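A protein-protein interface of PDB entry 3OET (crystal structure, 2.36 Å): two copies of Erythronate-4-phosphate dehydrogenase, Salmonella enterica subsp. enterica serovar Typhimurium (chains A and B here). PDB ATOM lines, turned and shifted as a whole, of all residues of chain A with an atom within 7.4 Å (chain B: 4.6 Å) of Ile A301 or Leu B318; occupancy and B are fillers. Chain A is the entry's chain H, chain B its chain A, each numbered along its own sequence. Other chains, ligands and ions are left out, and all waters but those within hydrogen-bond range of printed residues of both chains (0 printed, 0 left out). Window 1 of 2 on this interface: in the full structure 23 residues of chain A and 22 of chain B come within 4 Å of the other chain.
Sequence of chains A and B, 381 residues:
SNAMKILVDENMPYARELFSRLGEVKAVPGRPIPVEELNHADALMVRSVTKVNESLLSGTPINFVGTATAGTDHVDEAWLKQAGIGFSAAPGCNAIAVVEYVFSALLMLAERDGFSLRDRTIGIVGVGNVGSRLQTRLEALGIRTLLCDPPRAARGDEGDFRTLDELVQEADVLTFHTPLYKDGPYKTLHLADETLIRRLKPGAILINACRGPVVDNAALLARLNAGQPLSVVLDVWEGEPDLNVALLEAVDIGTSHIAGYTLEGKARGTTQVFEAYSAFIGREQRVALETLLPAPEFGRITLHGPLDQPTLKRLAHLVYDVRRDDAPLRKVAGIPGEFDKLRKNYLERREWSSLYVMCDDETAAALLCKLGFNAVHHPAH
NH2 of Arg B314 lies within hydrogen-bond range of O of Leu A318 (2.6 Å).
O of Leu B318 lies within hydrogen-bond range of NH2 of Arg A314, 2.9 Å away.
N of Thr A302 sits at hydrogen-bond distance from O of Arg B300 (3.0 Å).
The backbone carbonyl oxygen (O) of Met A358 is in hydrogen-bond range of the backbone NH (N) of Leu A303, 2.9 Å away.
N of Met A358 lies within hydrogen-bond range of O of Ile A301.
The backbone carbonyl oxygen (O) of Tyr A356 lies within hydrogen-bond range of the backbone NH (N) of Ile A301 (3.1 Å).
CD1 of Phe A298 touches CD1 of Ile B301, at 3.6 Å.
Phe A298 touches Leu B315 (CE1 to CD2, 3.7 Å).
Ile B301 touches Arg A300.
CD1 of Ile A301 touches CD1 of Phe B298, 3.6 Å away.
O of Arg B300 touches CA of Ile A301, 3.2 Å away.
CD1 of Ile A301 touches CD1 of Ile B301 (3.9 Å).
Ile A301 touches Leu B318 (CD1 to CD2, 3.9 Å).
Thr A302 touches Phe B298 (O to CD1, 3.3 Å).
CD1 of Leu A303 touches CE1 of Phe B298 (3.8 Å).
NH2 of Arg A314 touches CD2 of Phe B298, at 3.7 Å.
Ile A301 touches four residues of chain B.
Of the printed residues of chain B, Thr A302 touches Phe B298 (3.3 Å) and Arg B300 (3.0 Å).
Of the printed residues of chain A, Phe B298 touches Ile A301, Thr A302, Leu A303, Thr A311, Arg A314 and Leu A315.
Of chain A, only Ile A301 (3.9 Å) and Arg A314 (2.9 Å) come within 4 Å of Leu B318.
Printed residues of chain A within 4 Å of Val B319: Arg A314 (3.9 Å).
The nearest printed residue of chain A that does not touch Ile B301 is Thr A302 (5.1 Å).
Of the 11 printed residues of chain B, 7 touch a printed residue of chain A.
Printed residues of chain B that touch a printed residue of chain A: Phe B298, Arg B300, Ile B301, Arg B314, Leu B315, Leu B318 and Val B319.
Hydrophobic or aromatic side chains of chain B within 4 Å of the printed part of chain A: Phe B298, Ile B301, Leu B315 and Leu B318.
Among the printed residues, 18 pairs touch across the chains.
Among the printed residues, no Asp or Glu carboxylate lies within 4 Å of a Lys or Arg side-chain nitrogen of the other chain.
Phe A298 touches Ile B301, and with the chains exchanged Ile A301 touches Phe B298.
Phe A298 touches Leu B315, and with the chains exchanged Leu A315 touches Phe B298.
Ile B301 touches its own counterpart, Ile A301.
Ile A301 touches Leu B318, and with the chains exchanged Leu A318 touches Ile B301.
Positions printed for both chains: 298, 300, 301, 314, 315, 317, 318 and 355.
Of the 18 pairs that touch across the chains among the printed residues, 13 have their exchanged pair printed and touching as well.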
ATOM      1  N   PHE A 298     -10.661  18.615  -3.714  1.00  0.00           N
ATOM      2  CA  PHE A 298     -10.330  19.605  -4.741  1.00  0.00           C
ATOM      3  C   PHE A 298     -11.013  20.909  -4.415  1.00  0.00           C
ATOM      4  O   PHE A 298     -12.235  21.023  -4.532  1.00  0.00           O
ATOM      5  CB  PHE A 298     -10.762  19.150  -6.152  1.00  0.00           C
ATOM      6  CG  PHE A 298     -10.270  17.806  -6.505  1.00  0.00           C
ATOM      7  CD1 PHE A 298      -8.936  17.614  -6.793  1.00  0.00           C
ATOM      8  CD2 PHE A 298     -11.129  16.708  -6.489  1.00  0.00           C
ATOM      9  CE1 PHE A 298      -8.458  16.342  -7.102  1.00  0.00           C
ATOM     10  CE2 PHE A 298     -10.654  15.450  -6.791  1.00  0.00           C
ATOM     11  CZ  PHE A 298      -9.325  15.258  -7.097  1.00  0.00           C
ATOM     12  N   GLY A 299     -10.211  21.891  -4.028  1.00  0.00           N
ATOM     13  CA  GLY A 299     -10.735  23.161  -3.584  1.00  0.00           C
ATOM     14  C   GLY A 299     -10.516  24.294  -4.560  1.00  0.00           C
ATOM     15  O   GLY A 299     -11.173  25.320  -4.458  1.00  0.00           O
ATOM     16  N   ARG A 300      -9.607  24.134  -5.514  1.00  0.00           N
ATOM     17  CA  ARG A 300      -9.323  25.212  -6.462  1.00  0.00           C
ATOM     18  C   ARG A 300      -8.970  24.637  -7.797  1.00  0.00           C
ATOM     19  O   ARG A 300      -8.279  23.632  -7.834  1.00  0.00           O
ATOM     20  CB  ARG A 300      -8.095  25.987  -6.035  1.00  0.00           C
ATOM     21  CG  ARG A 300      -8.166  26.674  -4.730  1.00  0.00           C
ATOM     22  CD  ARG A 300      -7.335  27.923  -4.909  1.00  0.00           C
ATOM     23  NE  ARG A 300      -6.320  28.132  -3.893  1.00  0.00           N
ATOM     24  CZ  ARG A 300      -5.742  29.315  -3.714  1.00  0.00           C
ATOM     25  NH1 ARG A 300      -4.801  29.480  -2.779  1.00  0.00           N
ATOM     26  NH2 ARG A 300      -6.119  30.344  -4.480  1.00  0.00           N
ATOM     27  N   ILE A 301      -9.360  25.312  -8.880  1.00  0.00           N
ATOM     28  CA  ILE A 301      -9.059  24.856 -10.238  1.00  0.00           C
ATOM     29  C   ILE A 301      -9.068  26.063 -11.149  1.00  0.00           C
ATOM     30  O   ILE A 301      -9.800  26.999 -10.888  1.00  0.00           O
ATOM     31  CB  ILE A 301     -10.125  23.796 -10.747  1.00  0.00           C
ATOM     32  CG1 ILE A 301      -9.682  23.145 -12.052  1.00  0.00           C
ATOM     33  CG2 ILE A 301     -11.508  24.412 -10.956  1.00  0.00           C
ATOM     34  CD1 ILE A 301     -10.536  21.879 -12.386  1.00  0.00           C
ATOM     35  N   THR A 302      -8.247  26.060 -12.199  1.00  0.00           N
ATOM     36  CA  THR A 302      -8.309  27.125 -13.214  1.00  0.00           C
ATOM     37  C   THR A 302      -9.094  26.700 -14.456  1.00  0.00           C
ATOM     38  O   THR A 302      -9.041  25.535 -14.876  1.00  0.00           O
ATOM     39  CB  THR A 302      -6.922  27.634 -13.660  1.00  0.00           C
ATOM     40  OG1 THR A 302      -6.174  26.537 -14.171  1.00  0.00           O
ATOM     41  CG2 THR A 302      -6.171  28.241 -12.492  1.00  0.00           C
ATOM     42  N   LEU A 303      -9.846  27.651 -15.015  1.00  0.00           N
ATOM     43  CA  LEU A 303     -10.556  27.436 -16.274  1.00  0.00           C
ATOM     44  C   LEU A 303     -10.116  28.479 -17.299  1.00  0.00           C
ATOM     45  O   LEU A 303     -10.305  29.680 -17.108  1.00  0.00           O
ATOM     46  CB  LEU A 303     -12.085  27.445 -16.096  1.00  0.00           C
ATOM     47  CG  LEU A 303     -12.892  27.460 -17.415  1.00  0.00           C
ATOM     48  CD1 LEU A 303     -12.798  26.140 -18.202  1.00  0.00           C
ATOM     49  CD2 LEU A 303     -14.359  27.840 -17.207  1.00  0.00           C
ATOM     50  N   THR A 311     -17.422  21.384 -20.893  1.00  0.00           N
ATOM     51  CA  THR A 311     -16.618  21.952 -19.822  1.00  0.00           C
ATOM     52  C   THR A 311     -17.395  21.942 -18.521  1.00  0.00           C
ATOM     53  O   THR A 311     -16.843  21.614 -17.462  1.00  0.00           O
ATOM     54  CB  THR A 311     -16.197  23.410 -20.134  1.00  0.00           C
ATOM     55  OG1 THR A 311     -15.322  23.428 -21.269  1.00  0.00           O
ATOM     56  CG2 THR A 311     -15.459  24.006 -18.977  1.00  0.00           C
ATOM     57  N   LYS A 313     -19.771  19.914 -17.783  1.00  0.00           N
ATOM     58  CA  LYS A 313     -19.955  18.541 -17.309  1.00  0.00           C
ATOM     59  C   LYS A 313     -18.715  18.123 -16.537  1.00  0.00           C
ATOM     60  O   LYS A 313     -18.798  17.496 -15.474  1.00  0.00           O
ATOM     61  CB  LYS A 313     -20.193  17.548 -18.446  1.00  0.00           C
ATOM     62  CG  LYS A 313     -20.210  16.108 -17.949  1.00  0.00           C
ATOM     63  CD  LYS A 313     -20.416  15.093 -19.085  1.00  0.00           C
ATOM     64  CE  LYS A 313     -20.294  13.646 -18.578  1.00  0.00           C
ATOM     65  NZ  LYS A 313     -18.979  13.309 -17.916  1.00  0.00           N
ATOM     66  N   ARG A 314     -17.561  18.491 -17.073  1.00  0.00           N
ATOM     67  CA  ARG A 314     -16.341  18.152 -16.405  1.00  0.00           C
ATOM     68  C   ARG A 314     -16.272  18.762 -15.025  1.00  0.00           C
ATOM     69  O   ARG A 314     -15.807  18.113 -14.113  1.00  0.00           O
ATOM     70  CB  ARG A 314     -15.118  18.520 -17.237  1.00  0.00           C
ATOM     71  CG  ARG A 314     -14.907  17.572 -18.417  1.00  0.00           C
ATOM     72  CD  ARG A 314     -14.070  18.249 -19.508  1.00  0.00           C
ATOM     73  NE  ARG A 314     -12.636  18.068 -19.255  1.00  0.00           N
ATOM     74  CZ  ARG A 314     -11.653  18.660 -19.940  1.00  0.00           C
ATOM     75  NH1 ARG A 314     -11.904  19.523 -20.925  1.00  0.00           N
ATOM     76  NH2 ARG A 314     -10.399  18.373 -19.638  1.00  0.00           N
ATOM     77  N   LEU A 315     -16.717  20.005 -14.877  1.00  0.00           N
ATOM     78  CA  LEU A 315     -16.727  20.657 -13.550  1.00  0.00           C
ATOM     79  C   LEU A 315     -17.719  20.012 -12.559  1.00  0.00           C
ATOM     80  O   LEU A 315     -17.340  19.671 -11.429  1.00  0.00           O
ATOM     81  CB  LEU A 315     -16.983  22.177 -13.643  1.00  0.00           C
ATOM     82  CG  LEU A 315     -15.705  22.916 -14.032  1.00  0.00           C
ATOM     83  CD1 LEU A 315     -16.019  24.314 -14.585  1.00  0.00           C
ATOM     84  CD2 LEU A 315     -14.712  22.988 -12.846  1.00  0.00           C
ATOM     85  N   HIS A 317     -18.985  17.095 -12.635  1.00  0.00           N
ATOM     86  CA  HIS A 317     -18.636  15.711 -12.308  1.00  0.00           C
ATOM     87  C   HIS A 317     -17.329  15.572 -11.532  1.00  0.00           C
ATOM     88  O   HIS A 317     -17.162  14.602 -10.795  1.00  0.00           O
ATOM     89  CB  HIS A 317     -18.652  14.834 -13.549  1.00  0.00           C
ATOM     90  CG  HIS A 317     -20.034  14.472 -14.012  1.00  0.00           C
ATOM     91  ND1 HIS A 317     -20.265  13.572 -15.033  1.00  0.00           N
ATOM     92  CD2 HIS A 317     -21.257  14.863 -13.577  1.00  0.00           C
ATOM     93  CE1 HIS A 317     -21.571  13.439 -15.217  1.00  0.00           C
ATOM     94  NE2 HIS A 317     -22.196  14.215 -14.350  1.00  0.00           N
ATOM     95  N   LEU A 318     -16.406  16.533 -11.660  1.00  0.00           N
ATOM     96  CA  LEU A 318     -15.264  16.570 -10.733  1.00  0.00           C
ATOM     97  C   LEU A 318     -15.816  16.602  -9.308  1.00  0.00           C
ATOM     98  O   LEU A 318     -15.292  15.917  -8.417  1.00  0.00           O
ATOM     99  CB  LEU A 318     -14.397  17.807 -10.954  1.00  0.00           C
ATOM    100  CG  LEU A 318     -13.194  18.040 -10.031  1.00  0.00           C
ATOM    101  CD1 LEU A 318     -12.136  16.907 -10.163  1.00  0.00           C
ATOM    102  CD2 LEU A 318     -12.563  19.423 -10.355  1.00  0.00           C
ATOM    103  N   LEU A 355     -16.027  24.272  -4.728  1.00  0.00           N
ATOM    104  CA  LEU A 355     -14.975  24.386  -5.733  1.00  0.00           C
ATOM    105  C   LEU A 355     -14.762  25.862  -6.074  1.00  0.00           C
ATOM    106  O   LEU A 355     -15.689  26.564  -6.457  1.00  0.00           O
ATOM    107  CB  LEU A 355     -15.287  23.543  -6.993  1.00  0.00           C
ATOM    108  CG  LEU A 355     -14.156  23.377  -8.016  1.00  0.00           C
ATOM    109  CD1 LEU A 355     -12.953  22.754  -7.343  1.00  0.00           C
ATOM    110  CD2 LEU A 355     -14.561  22.510  -9.195  1.00  0.00           C
ATOM    111  N   TYR A 356     -13.539  26.331  -5.893  1.00  0.00           N
ATOM    112  CA  TYR A 356     -13.186  27.709  -6.203  1.00  0.00           C
ATOM    113  C   TYR A 356     -12.612  27.752  -7.616  1.00  0.00           C
ATOM    114  O   TYR A 356     -11.549  27.186  -7.871  1.00  0.00           O
ATOM    115  CB  TYR A 356     -12.183  28.202  -5.164  1.00  0.00           C
ATOM    116  CG  TYR A 356     -11.678  29.606  -5.369  1.00  0.00           C
ATOM    117  CD1 TYR A 356     -12.248  30.678  -4.704  1.00  0.00           C
ATOM    118  CD2 TYR A 356     -10.610  29.850  -6.205  1.00  0.00           C
ATOM    119  CE1 TYR A 356     -11.778  31.961  -4.875  1.00  0.00           C
ATOM    120  CE2 TYR A 356     -10.131  31.126  -6.392  1.00  0.00           C
ATOM    121  CZ  TYR A 356     -10.714  32.180  -5.726  1.00  0.00           C
ATOM    122  OH  TYR A 356     -10.200  33.439  -5.922  1.00  0.00           O
ATOM    123  N   VAL A 357     -13.334  28.396  -8.534  1.00  0.00           N
ATOM    124  CA  VAL A 357     -12.988  28.354  -9.961  1.00  0.00           C
ATOM    125  C   VAL A 357     -12.498  29.700 -10.524  1.00  0.00           C
ATOM    126  O   VAL A 357     -13.226  30.696 -10.522  1.00  0.00           O
ATOM    127  CB  VAL A 357     -14.173  27.837 -10.814  1.00  0.00           C
ATOM    128  CG1 VAL A 357     -13.766  27.724 -12.309  1.00  0.00           C
ATOM    129  CG2 VAL A 357     -14.606  26.507 -10.315  1.00  0.00           C
ATOM    130  N   MET A 358     -11.274  29.741 -11.021  1.00  0.00           N
ATOM    131  CA  MET A 358     -10.743  31.011 -11.512  1.00  0.00           C
ATOM    132  C   MET A 358     -10.686  31.009 -13.013  1.00  0.00           C
ATOM    133  O   MET A 358      -9.980  30.204 -13.597  1.00  0.00           O
ATOM    134  CB  MET A 358      -9.347  31.251 -10.975  1.00  0.00           C
ATOM    135  CG  MET A 358      -9.299  31.215  -9.488  1.00  0.00           C
ATOM    136  SD  MET A 358      -7.557  30.612  -8.858  1.00  0.00           S
ATOM    137  CE  MET A 358      -6.580  32.315  -9.058  1.00  0.00           C
ATOM    138  N   CYS A 359     -11.420  31.920 -13.628  1.00  0.00           N
ATOM    139  CA  CYS A 359     -11.588  31.898 -15.058  1.00  0.00           C
ATOM    140  C   CYS A 359     -10.943  33.111 -15.684  1.00  0.00           C
ATOM    141  O   CYS A 359     -11.128  34.237 -15.197  1.00  0.00           O
ATOM    142  CB  CYS A 359     -13.074  31.884 -15.393  1.00  0.00           C
ATOM    143  SG  CYS A 359     -13.994  30.763 -14.369  1.00  0.00           S
ATOM    144  N   PHE A 373     -21.069  27.591  -8.493  1.00  0.00           N
ATOM    145  CA  PHE A 373     -19.632  27.520  -8.258  1.00  0.00           C
ATOM    146  C   PHE A 373     -19.170  28.822  -7.618  1.00  0.00           C
ATOM    147  O   PHE A 373     -19.786  29.863  -7.795  1.00  0.00           O
ATOM    148  CB  PHE A 373     -18.865  27.282  -9.578  1.00  0.00           C
ATOM    149  CG  PHE A 373     -19.161  25.939 -10.178  1.00  0.00           C
ATOM    150  CD1 PHE A 373     -18.430  24.826  -9.793  1.00  0.00           C
ATOM    151  CD2 PHE A 373     -20.235  25.779 -11.041  1.00  0.00           C
ATOM    152  CE1 PHE A 373     -18.732  23.566 -10.295  1.00  0.00           C
ATOM    153  CE2 PHE A 373     -20.546  24.533 -11.543  1.00  0.00           C
ATOM    154  CZ  PHE A 373     -19.790  23.414 -11.164  1.00  0.00           C
ATOM    155  N   ASN A 374     -18.082  28.743  -6.872  1.00  0.00           N
ATOM    156  CA  ASN A 374     -17.437  29.925  -6.337  1.00  0.00           C
ATOM    157  C   ASN A 374     -16.392  30.354  -7.365  1.00  0.00           C
ATOM    158  O   ASN A 374     -15.209  30.042  -7.249  1.00  0.00           O
ATOM    159  CB  ASN A 374     -16.811  29.575  -5.000  1.00  0.00           C
ATOM    160  CG  ASN A 374     -16.171  30.756  -4.322  1.00  0.00           C
ATOM    161  OD1 ASN A 374     -16.487  31.926  -4.607  1.00  0.00           O
ATOM    162  ND2 ASN A 374     -15.253  30.459  -3.406  1.00  0.00           N
ATOM    163  N   VAL A 376     -14.471  33.138  -9.983  1.00  0.00           N
ATOM    164  CA  VAL A 376     -13.974  34.512  -9.978  1.00  0.00           C
ATOM    165  C   VAL A 376     -13.102  34.748 -11.193  1.00  0.00           C
ATOM    166  O   VAL A 376     -12.378  33.851 -11.643  1.00  0.00           O
ATOM    167  CB  VAL A 376     -13.182  34.876  -8.688  1.00  0.00           C
ATOM    168  CG1 VAL A 376     -14.082  34.809  -7.449  1.00  0.00           C
ATOM    169  CG2 VAL A 376     -11.978  33.978  -8.518  1.00  0.00           C
ATOM    170  N   PHE B 298      -8.417  23.050 -18.411  1.00  0.00           N
ATOM    171  CA  PHE B 298      -8.117  22.983 -16.985  1.00  0.00           C
ATOM    172  C   PHE B 298      -6.644  22.779 -16.832  1.00  0.00           C
ATOM    173  O   PHE B 298      -6.126  21.715 -17.167  1.00  0.00           O
ATOM    174  CB  PHE B 298      -8.867  21.843 -16.288  1.00  0.00           C
ATOM    175  CG  PHE B 298     -10.336  21.958 -16.412  1.00  0.00           C
ATOM    176  CD1 PHE B 298     -11.019  23.003 -15.770  1.00  0.00           C
ATOM    177  CD2 PHE B 298     -11.049  21.073 -17.210  1.00  0.00           C
ATOM    178  CE1 PHE B 298     -12.388  23.143 -15.906  1.00  0.00           C
ATOM    179  CE2 PHE B 298     -12.434  21.214 -17.337  1.00  0.00           C
ATOM    180  CZ  PHE B 298     -13.094  22.260 -16.680  1.00  0.00           C
ATOM    181  N   ARG B 300      -4.697  23.919 -13.857  1.00  0.00           N
ATOM    182  CA  ARG B 300      -4.162  23.795 -12.519  1.00  0.00           C
ATOM    183  C   ARG B 300      -5.238  23.378 -11.557  1.00  0.00           C
ATOM    184  O   ARG B 300      -6.349  23.822 -11.689  1.00  0.00           O
ATOM    185  CB  ARG B 300      -3.545  25.141 -12.087  1.00  0.00           C
ATOM    186  CG  ARG B 300      -2.167  25.317 -12.641  1.00  0.00           C
ATOM    187  CD  ARG B 300      -1.705  26.774 -12.692  1.00  0.00           C
ATOM    188  NE  ARG B 300      -2.220  27.541 -11.568  1.00  0.00           N
ATOM    189  CZ  ARG B 300      -2.013  28.838 -11.429  1.00  0.00           C
ATOM    190  NH1 ARG B 300      -1.282  29.462 -12.348  1.00  0.00           N
ATOM    191  NH2 ARG B 300      -2.532  29.497 -10.392  1.00  0.00           N
ATOM    192  N   ILE B 301      -4.898  22.547 -10.580  1.00  0.00           N
ATOM    193  CA  ILE B 301      -5.842  22.084  -9.592  1.00  0.00           C
ATOM    194  C   ILE B 301      -5.080  21.744  -8.301  1.00  0.00           C
ATOM    195  O   ILE B 301      -3.935  21.278  -8.350  1.00  0.00           O
ATOM    196  CB  ILE B 301      -6.652  20.852 -10.141  1.00  0.00           C
ATOM    197  CG1 ILE B 301      -7.842  20.492  -9.250  1.00  0.00           C
ATOM    198  CG2 ILE B 301      -5.753  19.623 -10.366  1.00  0.00           C
ATOM    199  CD1 ILE B 301      -8.773  19.407  -9.905  1.00  0.00           C
ATOM    200  N   ARG B 314     -11.171  10.620 -10.341  1.00  0.00           N
ATOM    201  CA  ARG B 314     -11.575  12.000 -10.611  1.00  0.00           C
ATOM    202  C   ARG B 314     -10.502  12.821 -11.343  1.00  0.00           C
ATOM    203  O   ARG B 314     -10.808  13.602 -12.258  1.00  0.00           O
ATOM    204  CB  ARG B 314     -11.983  12.698  -9.309  1.00  0.00           C
ATOM    205  CG  ARG B 314     -13.113  11.971  -8.617  1.00  0.00           C
ATOM    206  CD  ARG B 314     -13.245  12.375  -7.185  1.00  0.00           C
ATOM    207  NE  ARG B 314     -13.858  13.686  -7.066  1.00  0.00           N
ATOM    208  CZ  ARG B 314     -14.019  14.348  -5.919  1.00  0.00           C
ATOM    209  NH1 ARG B 314     -13.585  13.827  -4.784  1.00  0.00           N
ATOM    210  NH2 ARG B 314     -14.599  15.547  -5.909  1.00  0.00           N
ATOM    211  N   LEU B 315      -9.244  12.640 -10.973  1.00  0.00           N
ATOM    212  CA  LEU B 315      -8.168  13.282 -11.731  1.00  0.00           C
ATOM    213  C   LEU B 315      -8.048  12.824 -13.190  1.00  0.00           C
ATOM    214  O   LEU B 315      -8.030  13.626 -14.082  1.00  0.00           O
ATOM    215  CB  LEU B 315      -6.837  13.103 -11.022  1.00  0.00           C
ATOM    216  CG  LEU B 315      -6.684  14.010  -9.798  1.00  0.00           C
ATOM    217  CD1 LEU B 315      -5.447  13.574  -9.050  1.00  0.00           C
ATOM    218  CD2 LEU B 315      -6.575  15.518 -10.185  1.00  0.00           C
ATOM    219  N   ALA B 316      -7.937  11.541 -13.449  1.00  0.00           N
ATOM    220  CA  ALA B 316      -7.783  11.085 -14.828  1.00  0.00           C
ATOM    221  C   ALA B 316      -8.975  11.470 -15.685  1.00  0.00           C
ATOM    222  O   ALA B 316      -8.843  11.881 -16.830  1.00  0.00           O
ATOM    223  CB  ALA B 316      -7.603   9.591 -14.858  1.00  0.00           C
ATOM    224  N   HIS B 317     -10.159  11.336 -15.114  1.00  0.00           N
ATOM    225  CA  HIS B 317     -11.390  11.541 -15.897  1.00  0.00           C
ATOM    226  C   HIS B 317     -11.671  13.013 -16.102  1.00  0.00           C
ATOM    227  O   HIS B 317     -12.383  13.388 -17.023  1.00  0.00           O
ATOM    228  CB  HIS B 317     -12.554  10.850 -15.228  1.00  0.00           C
ATOM    229  CG  HIS B 317     -12.613   9.385 -15.504  1.00  0.00           C
ATOM    230  ND1 HIS B 317     -13.711   8.607 -15.184  1.00  0.00           N
ATOM    231  CD2 HIS B 317     -11.727   8.556 -16.102  1.00  0.00           C
ATOM    232  CE1 HIS B 317     -13.499   7.365 -15.577  1.00  0.00           C
ATOM    233  NE2 HIS B 317     -12.299   7.303 -16.128  1.00  0.00           N
ATOM    234  N   LEU B 318     -11.078  13.855 -15.266  1.00  0.00           N
ATOM    235  CA  LEU B 318     -11.135  15.289 -15.533  1.00  0.00           C
ATOM    236  C   LEU B 318     -10.419  15.551 -16.829  1.00  0.00           C
ATOM    237  O   LEU B 318     -10.863  16.371 -17.629  1.00  0.00           O
ATOM    238  CB  LEU B 318     -10.497  16.102 -14.421  1.00  0.00           C
ATOM    239  CG  LEU B 318     -10.403  17.601 -14.692  1.00  0.00           C
ATOM    240  CD1 LEU B 318     -11.757  18.277 -14.940  1.00  0.00           C
ATOM    241  CD2 LEU B 318      -9.654  18.258 -13.519  1.00  0.00           C
ATOM    242  N   VAL B 319      -9.332  14.832 -17.062  1.00  0.00           N
ATOM    243  CA  VAL B 319      -8.608  14.992 -18.320  1.00  0.00           C
ATOM    244  C   VAL B 319      -9.199  14.198 -19.499  1.00  0.00           C
ATOM    245  O   VAL B 319      -9.403  14.742 -20.611  1.00  0.00           O
ATOM    246  CB  VAL B 319      -7.127  14.597 -18.189  1.00  0.00           C
ATOM    247  CG1 VAL B 319      -6.429  14.796 -19.558  1.00  0.00           C
ATOM    248  CG2 VAL B 319      -6.408  15.403 -17.059  1.00  0.00           C
ATOM    249  N   TYR B 320      -9.431  12.913 -19.272  1.00  0.00           N
ATOM    250  CA  TYR B 320     -10.020  12.061 -20.274  1.00  0.00           C
ATOM    251  C   TYR B 320     -10.818  10.903 -19.688  1.00  0.00           C
ATOM    252  O   TYR B 320     -10.264  10.032 -19.003  1.00  0.00           O
ATOM    253  CB  TYR B 320      -8.935  11.515 -21.193  1.00  0.00           C
ATOM    254  CG  TYR B 320      -9.492  10.576 -22.215  1.00  0.00           C
ATOM    255  CD1 TYR B 320     -10.467  11.007 -23.120  1.00  0.00           C
ATOM    256  CD2 TYR B 320      -9.058   9.255 -22.277  1.00  0.00           C
ATOM    257  CE1 TYR B 320     -11.006  10.142 -24.068  1.00  0.00           C
ATOM    258  CE2 TYR B 320      -9.579   8.368 -23.213  1.00  0.00           C
ATOM    259  CZ  TYR B 320     -10.549   8.824 -24.108  1.00  0.00           C
ATOM    260  OH  TYR B 320     -11.042   7.964 -25.044  1.00  0.00           O
ATOM    261  N   LEU B 355      -1.977  18.759 -16.915  1.00  0.00           N
ATOM    262  CA  LEU B 355      -2.707  19.142 -15.707  1.00  0.00           C
ATOM    263  C   LEU B 355      -1.721  19.250 -14.560  1.00  0.00           C
ATOM    264  O   LEU B 355      -1.063  18.253 -14.158  1.00  0.00           O
ATOM    265  CB  LEU B 355      -3.824  18.124 -15.336  1.00  0.00           C
ATOM    266  CG  LEU B 355      -4.667  18.467 -14.067  1.00  0.00           C
ATOM    267  CD1 LEU B 355      -5.493  19.782 -14.192  1.00  0.00           C
ATOM    268  CD2 LEU B 355      -5.604  17.347 -13.613  1.00  0.00           C
